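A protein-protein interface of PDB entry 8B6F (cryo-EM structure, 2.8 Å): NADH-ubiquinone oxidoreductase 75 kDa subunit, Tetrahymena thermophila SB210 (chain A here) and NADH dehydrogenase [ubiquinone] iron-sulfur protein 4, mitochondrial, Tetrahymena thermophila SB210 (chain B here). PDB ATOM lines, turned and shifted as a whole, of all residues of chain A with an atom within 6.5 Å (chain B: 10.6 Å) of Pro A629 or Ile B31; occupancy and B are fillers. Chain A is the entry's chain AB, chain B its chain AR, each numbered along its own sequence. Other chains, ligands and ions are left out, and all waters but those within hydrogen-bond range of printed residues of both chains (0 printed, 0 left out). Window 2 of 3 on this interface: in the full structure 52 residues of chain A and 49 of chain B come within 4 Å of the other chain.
The backbone carbonyl oxygen (O) of Leu B32 lies close to the side-chain carboxylate (OE2) of Glu A642, 3.4 Å away.
The backbone carbonyl oxygen of Pro A629 sits close to the side-chain amide oxygen of Asn B28, 3.0 Å away.
OE2 of Glu A642 sits close to N of Val B34, 3.5 Å away.
The side-chain carboxylate (OD2) of Asp A631 is in hydrogen-bond range of the side-chain amide nitrogen (ND2) of Asn B28, at 3.2 Å.
ND2 of Asn B28 sits at hydrogen-bond distance from OE1 of Glu A635, 3.0 Å away.
The backbone NH (N) of Gly B35 sits at hydrogen-bond distance from the side-chain carboxylate (OE2) of Glu A642 (2.6 Å).
The side-chain carboxylate of Asp A357 lies within salt-bridge range of the guanidinium group of Arg A639, 3.4 Å away.
The side-chain carboxylate of Glu A635 lies within hydrogen-bond range of the backbone NH of Asp A631 (2.6 Å).
NH2 of Arg A618 lies within salt-bridge range of OD1 of Asp A631.
Among the printed residues, merely in contact across the chains: Glu A635 with Leu B32, Pro A629 with Leu B32, Arg A639 with Leu B32 and Pro A629 with Ile B31.
Of the printed residues of chain B, Pro A629 touches Asn B28, Ile B31 and Leu B32.
Ile B31 touches just one residue of chain A: Pro A629.
No residue of chain B comes within 4 Å of Tyr A630.
Printed residues of chain B within 4 Å of Asp A631: Asn B28.
Of the printed residues of chain A, Asn B28 touches Pro A629, Asp A631 and Glu A635.
Of the printed residues of chain A, Gly B35 touches Glu A642 (2.6 Å).
Of the printed residues of chain B, Glu A642 touches Leu B32, Val B34 and Gly B35.
Of the printed residues of chain B, Arg A639 touches Leu B32 (3.7 Å).
Ser B33 touches none of the printed residues of chain A.
Ala B24 touches none of the printed residues of chain A.
The nearest residue of chain B that does not touch Pro A629 is Glu B29 (5.2 Å).
The nearest residue of chain A that does not touch Ile B31 is Glu A642 (4.7 Å).
Hydrophobic or aromatic side chains of chain A within 4 Å of the printed part of chain B: Pro A629.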
ATOM      1  N   ASP A 357     -32.298   7.689  10.245  1.00  0.00           N
ATOM      2  CA  ASP A 357     -31.183   8.536   9.835  1.00  0.00           C
ATOM      3  C   ASP A 357     -31.676   9.869   9.289  1.00  0.00           C
ATOM      4  O   ASP A 357     -31.111  10.923   9.602  1.00  0.00           O
ATOM      5  CB  ASP A 357     -30.330   7.814   8.793  1.00  0.00           C
ATOM      6  CG  ASP A 357     -29.573   6.635   9.376  1.00  0.00           C
ATOM      7  OD1 ASP A 357     -29.726   6.367  10.585  1.00  0.00           O
ATOM      8  OD2 ASP A 357     -28.821   5.981   8.624  1.00  0.00           O
ATOM      9  N   ARG A 361     -30.865  13.490  10.968  1.00  0.00           N
ATOM     10  CA  ARG A 361     -30.225  14.574  10.234  1.00  0.00           C
ATOM     11  C   ARG A 361     -31.098  15.821  10.203  1.00  0.00           C
ATOM     12  O   ARG A 361     -30.577  16.936  10.092  1.00  0.00           O
ATOM     13  CB  ARG A 361     -29.887  14.116   8.817  1.00  0.00           C
ATOM     14  CG  ARG A 361     -28.611  13.292   8.731  1.00  0.00           C
ATOM     15  CD  ARG A 361     -28.434  12.696   7.346  1.00  0.00           C
ATOM     16  NE  ARG A 361     -27.082  12.195   7.130  1.00  0.00           N
ATOM     17  CZ  ARG A 361     -26.078  12.919   6.655  1.00  0.00           C
ATOM     18  NH1 ARG A 361     -26.231  14.196   6.344  1.00  0.00           N
ATOM     19  NH2 ARG A 361     -24.888  12.348   6.488  1.00  0.00           N
ATOM     20  N   ARG A 618     -34.088   7.849   0.959  1.00  0.00           N
ATOM     21  CA  ARG A 618     -32.787   8.311   0.490  1.00  0.00           C
ATOM     22  C   ARG A 618     -32.943   9.467  -0.490  1.00  0.00           C
ATOM     23  O   ARG A 618     -32.235  10.477  -0.397  1.00  0.00           O
ATOM     24  CB  ARG A 618     -32.031   7.143  -0.147  1.00  0.00           C
ATOM     25  CG  ARG A 618     -30.787   7.524  -0.937  1.00  0.00           C
ATOM     26  CD  ARG A 618     -29.764   8.235  -0.074  1.00  0.00           C
ATOM     27  NE  ARG A 618     -28.481   8.362  -0.754  1.00  0.00           N
ATOM     28  CZ  ARG A 618     -28.235   9.216  -1.739  1.00  0.00           C
ATOM     29  NH1 ARG A 618     -29.171  10.024  -2.203  1.00  0.00           N
ATOM     30  NH2 ARG A 618     -27.018   9.256  -2.272  1.00  0.00           N
ATOM     31  N   PRO A 627     -27.927  14.350   2.444  1.00  0.00           N
ATOM     32  CA  PRO A 627     -27.788  13.033   1.813  1.00  0.00           C
ATOM     33  C   PRO A 627     -27.336  11.969   2.801  1.00  0.00           C
ATOM     34  O   PRO A 627     -26.503  12.215   3.675  1.00  0.00           O
ATOM     35  CB  PRO A 627     -26.737  13.271   0.722  1.00  0.00           C
ATOM     36  CG  PRO A 627     -25.985  14.478   1.173  1.00  0.00           C
ATOM     37  CD  PRO A 627     -26.982  15.333   1.889  1.00  0.00           C
ATOM     38  N   LEU A 628     -27.905  10.766   2.652  1.00  0.00           N
ATOM     39  CA  LEU A 628     -27.534   9.637   3.489  1.00  0.00           C
ATOM     40  C   LEU A 628     -26.330   8.913   2.895  1.00  0.00           C
ATOM     41  O   LEU A 628     -26.117   8.946   1.679  1.00  0.00           O
ATOM     42  CB  LEU A 628     -28.702   8.669   3.630  1.00  0.00           C
ATOM     43  CG  LEU A 628     -29.979   9.287   4.204  1.00  0.00           C
ATOM     44  CD1 LEU A 628     -31.158   8.349   4.045  1.00  0.00           C
ATOM     45  CD2 LEU A 628     -29.787   9.637   5.667  1.00  0.00           C
ATOM     46  N   PRO A 629     -25.535   8.246   3.724  1.00  0.00           N
ATOM     47  CA  PRO A 629     -24.277   7.671   3.231  1.00  0.00           C
ATOM     48  C   PRO A 629     -24.429   6.323   2.541  1.00  0.00           C
ATOM     49  O   PRO A 629     -23.433   5.618   2.359  1.00  0.00           O
ATOM     50  CB  PRO A 629     -23.439   7.549   4.509  1.00  0.00           C
ATOM     51  CG  PRO A 629     -24.445   7.316   5.578  1.00  0.00           C
ATOM     52  CD  PRO A 629     -25.676   8.094   5.183  1.00  0.00           C
ATOM     53  N   TYR A 630     -25.647   5.939   2.165  1.00  0.00           N
ATOM     54  CA  TYR A 630     -25.885   4.665   1.495  1.00  0.00           C
ATOM     55  C   TYR A 630     -26.714   4.882   0.238  1.00  0.00           C
ATOM     56  O   TYR A 630     -27.765   5.527   0.286  1.00  0.00           O
ATOM     57  CB  TYR A 630     -26.586   3.674   2.428  1.00  0.00           C
ATOM     58  CG  TYR A 630     -27.520   4.320   3.419  1.00  0.00           C
ATOM     59  CD1 TYR A 630     -28.834   4.605   3.080  1.00  0.00           C
ATOM     60  CD2 TYR A 630     -27.085   4.639   4.698  1.00  0.00           C
ATOM     61  CE1 TYR A 630     -29.690   5.192   3.987  1.00  0.00           C
ATOM     62  CE2 TYR A 630     -27.931   5.226   5.611  1.00  0.00           C
ATOM     63  CZ  TYR A 630     -29.232   5.501   5.251  1.00  0.00           C
ATOM     64  OH  TYR A 630     -30.073   6.086   6.164  1.00  0.00           O
ATOM     65  N   ASP A 631     -26.238   4.330  -0.881  1.00  0.00           N
ATOM     66  CA  ASP A 631     -26.934   4.405  -2.157  1.00  0.00           C
ATOM     67  C   ASP A 631     -27.440   3.058  -2.650  1.00  0.00           C
ATOM     68  O   ASP A 631     -28.146   3.018  -3.664  1.00  0.00           O
ATOM     69  CB  ASP A 631     -26.015   5.008  -3.229  1.00  0.00           C
ATOM     70  CG  ASP A 631     -25.668   6.454  -2.953  1.00  0.00           C
ATOM     71  OD1 ASP A 631     -26.205   7.016  -1.976  1.00  0.00           O
ATOM     72  OD2 ASP A 631     -24.858   7.029  -3.710  1.00  0.00           O
ATOM     73  N   GLU A 635     -24.711  -0.919   1.050  1.00  0.00           N
ATOM     74  CA  GLU A 635     -24.284   0.182   1.905  1.00  0.00           C
ATOM     75  C   GLU A 635     -25.287   0.439   3.023  1.00  0.00           C
ATOM     76  O   GLU A 635     -24.899   0.762   4.150  1.00  0.00           O
ATOM     77  CB  GLU A 635     -24.069   1.440   1.066  1.00  0.00           C
ATOM     78  CG  GLU A 635     -23.012   1.265  -0.011  1.00  0.00           C
ATOM     79  CD  GLU A 635     -22.945   2.440  -0.960  1.00  0.00           C
ATOM     80  OE1 GLU A 635     -23.773   3.363  -0.824  1.00  0.00           O
ATOM     81  OE2 GLU A 635     -22.063   2.442  -1.841  1.00  0.00           O
ATOM     82  N   LEU A 636     -26.579   0.295   2.731  1.00  0.00           N
ATOM     83  CA  LEU A 636     -27.587   0.439   3.775  1.00  0.00           C
ATOM     84  C   LEU A 636     -27.414  -0.628   4.847  1.00  0.00           C
ATOM     85  O   LEU A 636     -27.571  -0.350   6.041  1.00  0.00           O
ATOM     86  CB  LEU A 636     -28.989   0.376   3.173  1.00  0.00           C
ATOM     87  CG  LEU A 636     -30.146   0.494   4.171  1.00  0.00           C
ATOM     88  CD1 LEU A 636     -29.971   1.671   5.119  1.00  0.00           C
ATOM     89  CD2 LEU A 636     -31.457   0.622   3.429  1.00  0.00           C
ATOM     90  N   ARG A 639     -24.657   0.345   7.088  1.00  0.00           N
ATOM     91  CA  ARG A 639     -25.156   1.250   8.116  1.00  0.00           C
ATOM     92  C   ARG A 639     -25.911   0.482   9.193  1.00  0.00           C
ATOM     93  O   ARG A 639     -25.798   0.789  10.385  1.00  0.00           O
ATOM     94  CB  ARG A 639     -26.053   2.315   7.488  1.00  0.00           C
ATOM     95  CG  ARG A 639     -26.486   3.409   8.451  1.00  0.00           C
ATOM     96  CD  ARG A 639     -25.311   4.289   8.849  1.00  0.00           C
ATOM     97  NE  ARG A 639     -25.714   5.376   9.733  1.00  0.00           N
ATOM     98  CZ  ARG A 639     -25.741   5.302  11.056  1.00  0.00           C
ATOM     99  NH1 ARG A 639     -25.399   4.197  11.696  1.00  0.00           N
ATOM    100  NH2 ARG A 639     -26.119   6.367  11.757  1.00  0.00           N
ATOM    101  N   GLU A 642     -23.428  -0.887  11.426  1.00  0.00           N
ATOM    102  CA  GLU A 642     -22.991   0.159  12.343  1.00  0.00           C
ATOM    103  C   GLU A 642     -23.931   0.262  13.540  1.00  0.00           C
ATOM    104  O   GLU A 642     -23.491   0.292  14.694  1.00  0.00           O
ATOM    105  CB  GLU A 642     -22.930   1.498  11.607  1.00  0.00           C
ATOM    106  CG  GLU A 642     -21.915   1.554  10.482  1.00  0.00           C
ATOM    107  CD  GLU A 642     -20.555   2.007  10.951  1.00  0.00           C
ATOM    108  OE1 GLU A 642     -20.276   1.898  12.163  1.00  0.00           O
ATOM    109  OE2 GLU A 642     -19.763   2.474  10.107  1.00  0.00           O
ATOM    110  N   ILE B  23     -12.969  -4.411   0.995  1.00  0.00           N
ATOM    111  CA  ILE B  23     -12.110  -3.250   1.189  1.00  0.00           C
ATOM    112  C   ILE B  23     -12.906  -2.024   0.761  1.00  0.00           C
ATOM    113  O   ILE B  23     -13.382  -1.955  -0.379  1.00  0.00           O
ATOM    114  CB  ILE B  23     -10.805  -3.363   0.385  1.00  0.00           C
ATOM    115  CG1 ILE B  23     -10.058  -4.651   0.745  1.00  0.00           C
ATOM    116  CG2 ILE B  23      -9.923  -2.143   0.620  1.00  0.00           C
ATOM    117  CD1 ILE B  23      -9.674  -4.772   2.206  1.00  0.00           C
ATOM    118  N   ALA B  24     -13.051  -1.066   1.670  1.00  0.00           N
ATOM    119  CA  ALA B  24     -13.835   0.127   1.382  1.00  0.00           C
ATOM    120  C   ALA B  24     -13.203   0.913   0.242  1.00  0.00           C
ATOM    121  O   ALA B  24     -12.062   1.373   0.351  1.00  0.00           O
ATOM    122  CB  ALA B  24     -13.944   0.997   2.633  1.00  0.00           C
ATOM    123  N   LYS B  25     -13.945   1.061  -0.853  1.00  0.00           N
ATOM    124  CA  LYS B  25     -13.486   1.797  -2.024  1.00  0.00           C
ATOM    125  C   LYS B  25     -14.341   3.020  -2.313  1.00  0.00           C
ATOM    126  O   LYS B  25     -13.804   4.123  -2.472  1.00  0.00           O
ATOM    127  CB  LYS B  25     -13.464   0.869  -3.248  1.00  0.00           C
ATOM    128  CG  LYS B  25     -12.917   1.525  -4.511  1.00  0.00           C
ATOM    129  CD  LYS B  25     -12.788   0.529  -5.656  1.00  0.00           C
ATOM    130  CE  LYS B  25     -14.145   0.034  -6.132  1.00  0.00           C
ATOM    131  NZ  LYS B  25     -14.021  -0.900  -7.287  1.00  0.00           N
ATOM    132  N   THR B  26     -15.658   2.858  -2.384  1.00  0.00           N
ATOM    133  CA  THR B  26     -16.538   3.980  -2.666  1.00  0.00           C
ATOM    134  C   THR B  26     -16.517   4.973  -1.506  1.00  0.00           C
ATOM    135  O   THR B  26     -16.138   4.648  -0.378  1.00  0.00           O
ATOM    136  CB  THR B  26     -17.964   3.483  -2.916  1.00  0.00           C
ATOM    137  OG1 THR B  26     -17.942   2.427  -3.884  1.00  0.00           O
ATOM    138  CG2 THR B  26     -18.866   4.600  -3.432  1.00  0.00           C
ATOM    139  N   ALA B  27     -16.930   6.207  -1.799  1.00  0.00           N
ATOM    140  CA  ALA B  27     -16.989   7.230  -0.762  1.00  0.00           C
ATOM    141  C   ALA B  27     -17.951   6.826   0.346  1.00  0.00           C
ATOM    142  O   ALA B  27     -17.663   7.020   1.532  1.00  0.00           O
ATOM    143  CB  ALA B  27     -17.402   8.569  -1.370  1.00  0.00           C
ATOM    144  N   ASN B  28     -19.102   6.262  -0.023  1.00  0.00           N
ATOM    145  CA  ASN B  28     -20.048   5.791   0.981  1.00  0.00           C
ATOM    146  C   ASN B  28     -19.437   4.695   1.842  1.00  0.00           C
ATOM    147  O   ASN B  28     -19.604   4.691   3.067  1.00  0.00           O
ATOM    148  CB  ASN B  28     -21.318   5.286   0.300  1.00  0.00           C
ATOM    149  CG  ASN B  28     -22.201   6.414  -0.195  1.00  0.00           C
ATOM    150  OD1 ASN B  28     -22.248   7.489   0.402  1.00  0.00           O
ATOM    151  ND2 ASN B  28     -22.907   6.174  -1.294  1.00  0.00           N
ATOM    152  N   GLU B  29     -18.722   3.757   1.221  1.00  0.00           N
ATOM    153  CA  GLU B  29     -18.083   2.690   1.984  1.00  0.00           C
ATOM    154  C   GLU B  29     -17.033   3.249   2.935  1.00  0.00           C
ATOM    155  O   GLU B  29     -16.925   2.802   4.083  1.00  0.00           O
ATOM    156  CB  GLU B  29     -17.466   1.668   1.031  1.00  0.00           C
ATOM    157  CG  GLU B  29     -18.483   1.017   0.105  1.00  0.00           C
ATOM    158  CD  GLU B  29     -17.844   0.085  -0.906  1.00  0.00           C
ATOM    159  OE1 GLU B  29     -16.599  -0.002  -0.934  1.00  0.00           O
ATOM    160  OE2 GLU B  29     -18.587  -0.563  -1.671  1.00  0.00           O
ATOM    161  N   LYS B  30     -16.246   4.225   2.478  1.00  0.00           N
ATOM    162  CA  LYS B  30     -15.257   4.844   3.353  1.00  0.00           C
ATOM    163  C   LYS B  30     -15.929   5.552   4.523  1.00  0.00           C
ATOM    164  O   LYS B  30     -15.444   5.485   5.659  1.00  0.00           O
ATOM    165  CB  LYS B  30     -14.387   5.817   2.559  1.00  0.00           C
ATOM    166  CG  LYS B  30     -13.468   5.137   1.557  1.00  0.00           C
ATOM    167  CD  LYS B  30     -12.600   6.148   0.825  1.00  0.00           C
ATOM    168  CE  LYS B  30     -11.638   5.463  -0.131  1.00  0.00           C
ATOM    169  NZ  LYS B  30     -10.760   6.442  -0.831  1.00  0.00           N
ATOM    170  N   ILE B  31     -17.042   6.238   4.265  1.00  0.00           N
ATOM    171  CA  ILE B  31     -17.785   6.881   5.346  1.00  0.00           C
ATOM    172  C   ILE B  31     -18.270   5.838   6.343  1.00  0.00           C
ATOM    173  O   ILE B  31     -18.248   6.061   7.559  1.00  0.00           O
ATOM    174  CB  ILE B  31     -18.953   7.706   4.772  1.00  0.00           C
ATOM    175  CG1 ILE B  31     -18.418   8.886   3.960  1.00  0.00           C
ATOM    176  CG2 ILE B  31     -19.860   8.206   5.890  1.00  0.00           C
ATOM    177  CD1 ILE B  31     -19.465   9.561   3.102  1.00  0.00           C
ATOM    178  N   LEU B  32     -18.722   4.687   5.844  1.00  0.00           N
ATOM    179  CA  LEU B  32     -19.193   3.589   6.679  1.00  0.00           C
ATOM    180  C   LEU B  32     -18.096   2.576   6.979  1.00  0.00           C
ATOM    181  O   LEU B  32     -18.391   1.395   7.207  1.00  0.00           O
ATOM    182  CB  LEU B  32     -20.380   2.901   6.004  1.00  0.00           C
ATOM    183  CG  LEU B  32     -21.527   3.827   5.597  1.00  0.00           C
ATOM    184  CD1 LEU B  32     -22.549   3.086   4.753  1.00  0.00           C
ATOM    185  CD2 LEU B  32     -22.186   4.434   6.823  1.00  0.00           C
ATOM    186  N   SER B  33     -16.832   3.009   6.974  1.00  0.00           N
ATOM    187  CA  SER B  33     -15.718   2.085   7.164  1.00  0.00           C
ATOM    188  C   SER B  33     -15.904   1.221   8.404  1.00  0.00           C
ATOM    189  O   SER B  33     -15.596   0.025   8.387  1.00  0.00           O
ATOM    190  CB  SER B  33     -14.406   2.864   7.251  1.00  0.00           C
ATOM    191  OG  SER B  33     -14.431   3.795   8.318  1.00  0.00           O
ATOM    192  N   VAL B  34     -16.398   1.808   9.496  1.00  0.00           N
ATOM    193  CA  VAL B  34     -16.621   1.025  10.707  1.00  0.00           C
ATOM    194  C   VAL B  34     -17.609  -0.099  10.432  1.00  0.00           C
ATOM    195  O   VAL B  34     -17.451  -1.221  10.927  1.00  0.00           O
ATOM    196  CB  VAL B  34     -17.099   1.934  11.856  1.00  0.00           C
ATOM    197  CG1 VAL B  34     -17.441   1.113  13.092  1.00  0.00           C
ATOM    198  CG2 VAL B  34     -16.039   2.972  12.185  1.00  0.00           C
ATOM    199  N   GLY B  35     -18.644   0.182   9.639  1.00  0.00           N
ATOM    200  CA  GLY B  35     -19.592  -0.860   9.287  1.00  0.00           C
ATOM    201  C   GLY B  35     -18.955  -1.978   8.488  1.00  0.00           C
ATOM    202  O   GLY B  35     -19.246  -3.157   8.708  1.00  0.00           O
ATOM    203  N   VAL B  36     -18.078  -1.627   7.545  1.00  0.00           N
ATOM    204  CA  VAL B  36     -17.388  -2.645   6.759  1.00  0.00           C
ATOM    205  C   VAL B  36     -16.517  -3.509   7.661  1.00  0.00           C
ATOM    206  O   VAL B  36     -16.482  -4.737   7.526  1.00  0.00           O
ATOM    207  CB  VAL B  36     -16.567  -1.987   5.634  1.00  0.00           C
ATOM    208  CG1 VAL B  36     -15.793  -3.036   4.850  1.00  0.00           C
ATOM    209  CG2 VAL B  36     -17.477  -1.194   4.709  1.00  0.00           C
ATOM    210  N   ALA B  37     -15.799  -2.881   8.594  1.00  0.00           N
ATOM    211  CA  ALA B  37     -14.964  -3.644   9.515  1.00  0.00           C
ATOM    212  C   ALA B  37     -15.804  -4.577  10.376  1.00  0.00           C
ATOM    213  O   ALA B  37     -15.431  -5.735  10.593  1.00  0.00           O
ATOM    214  CB  ALA B  37     -14.149  -2.693  10.391  1.00  0.00           C
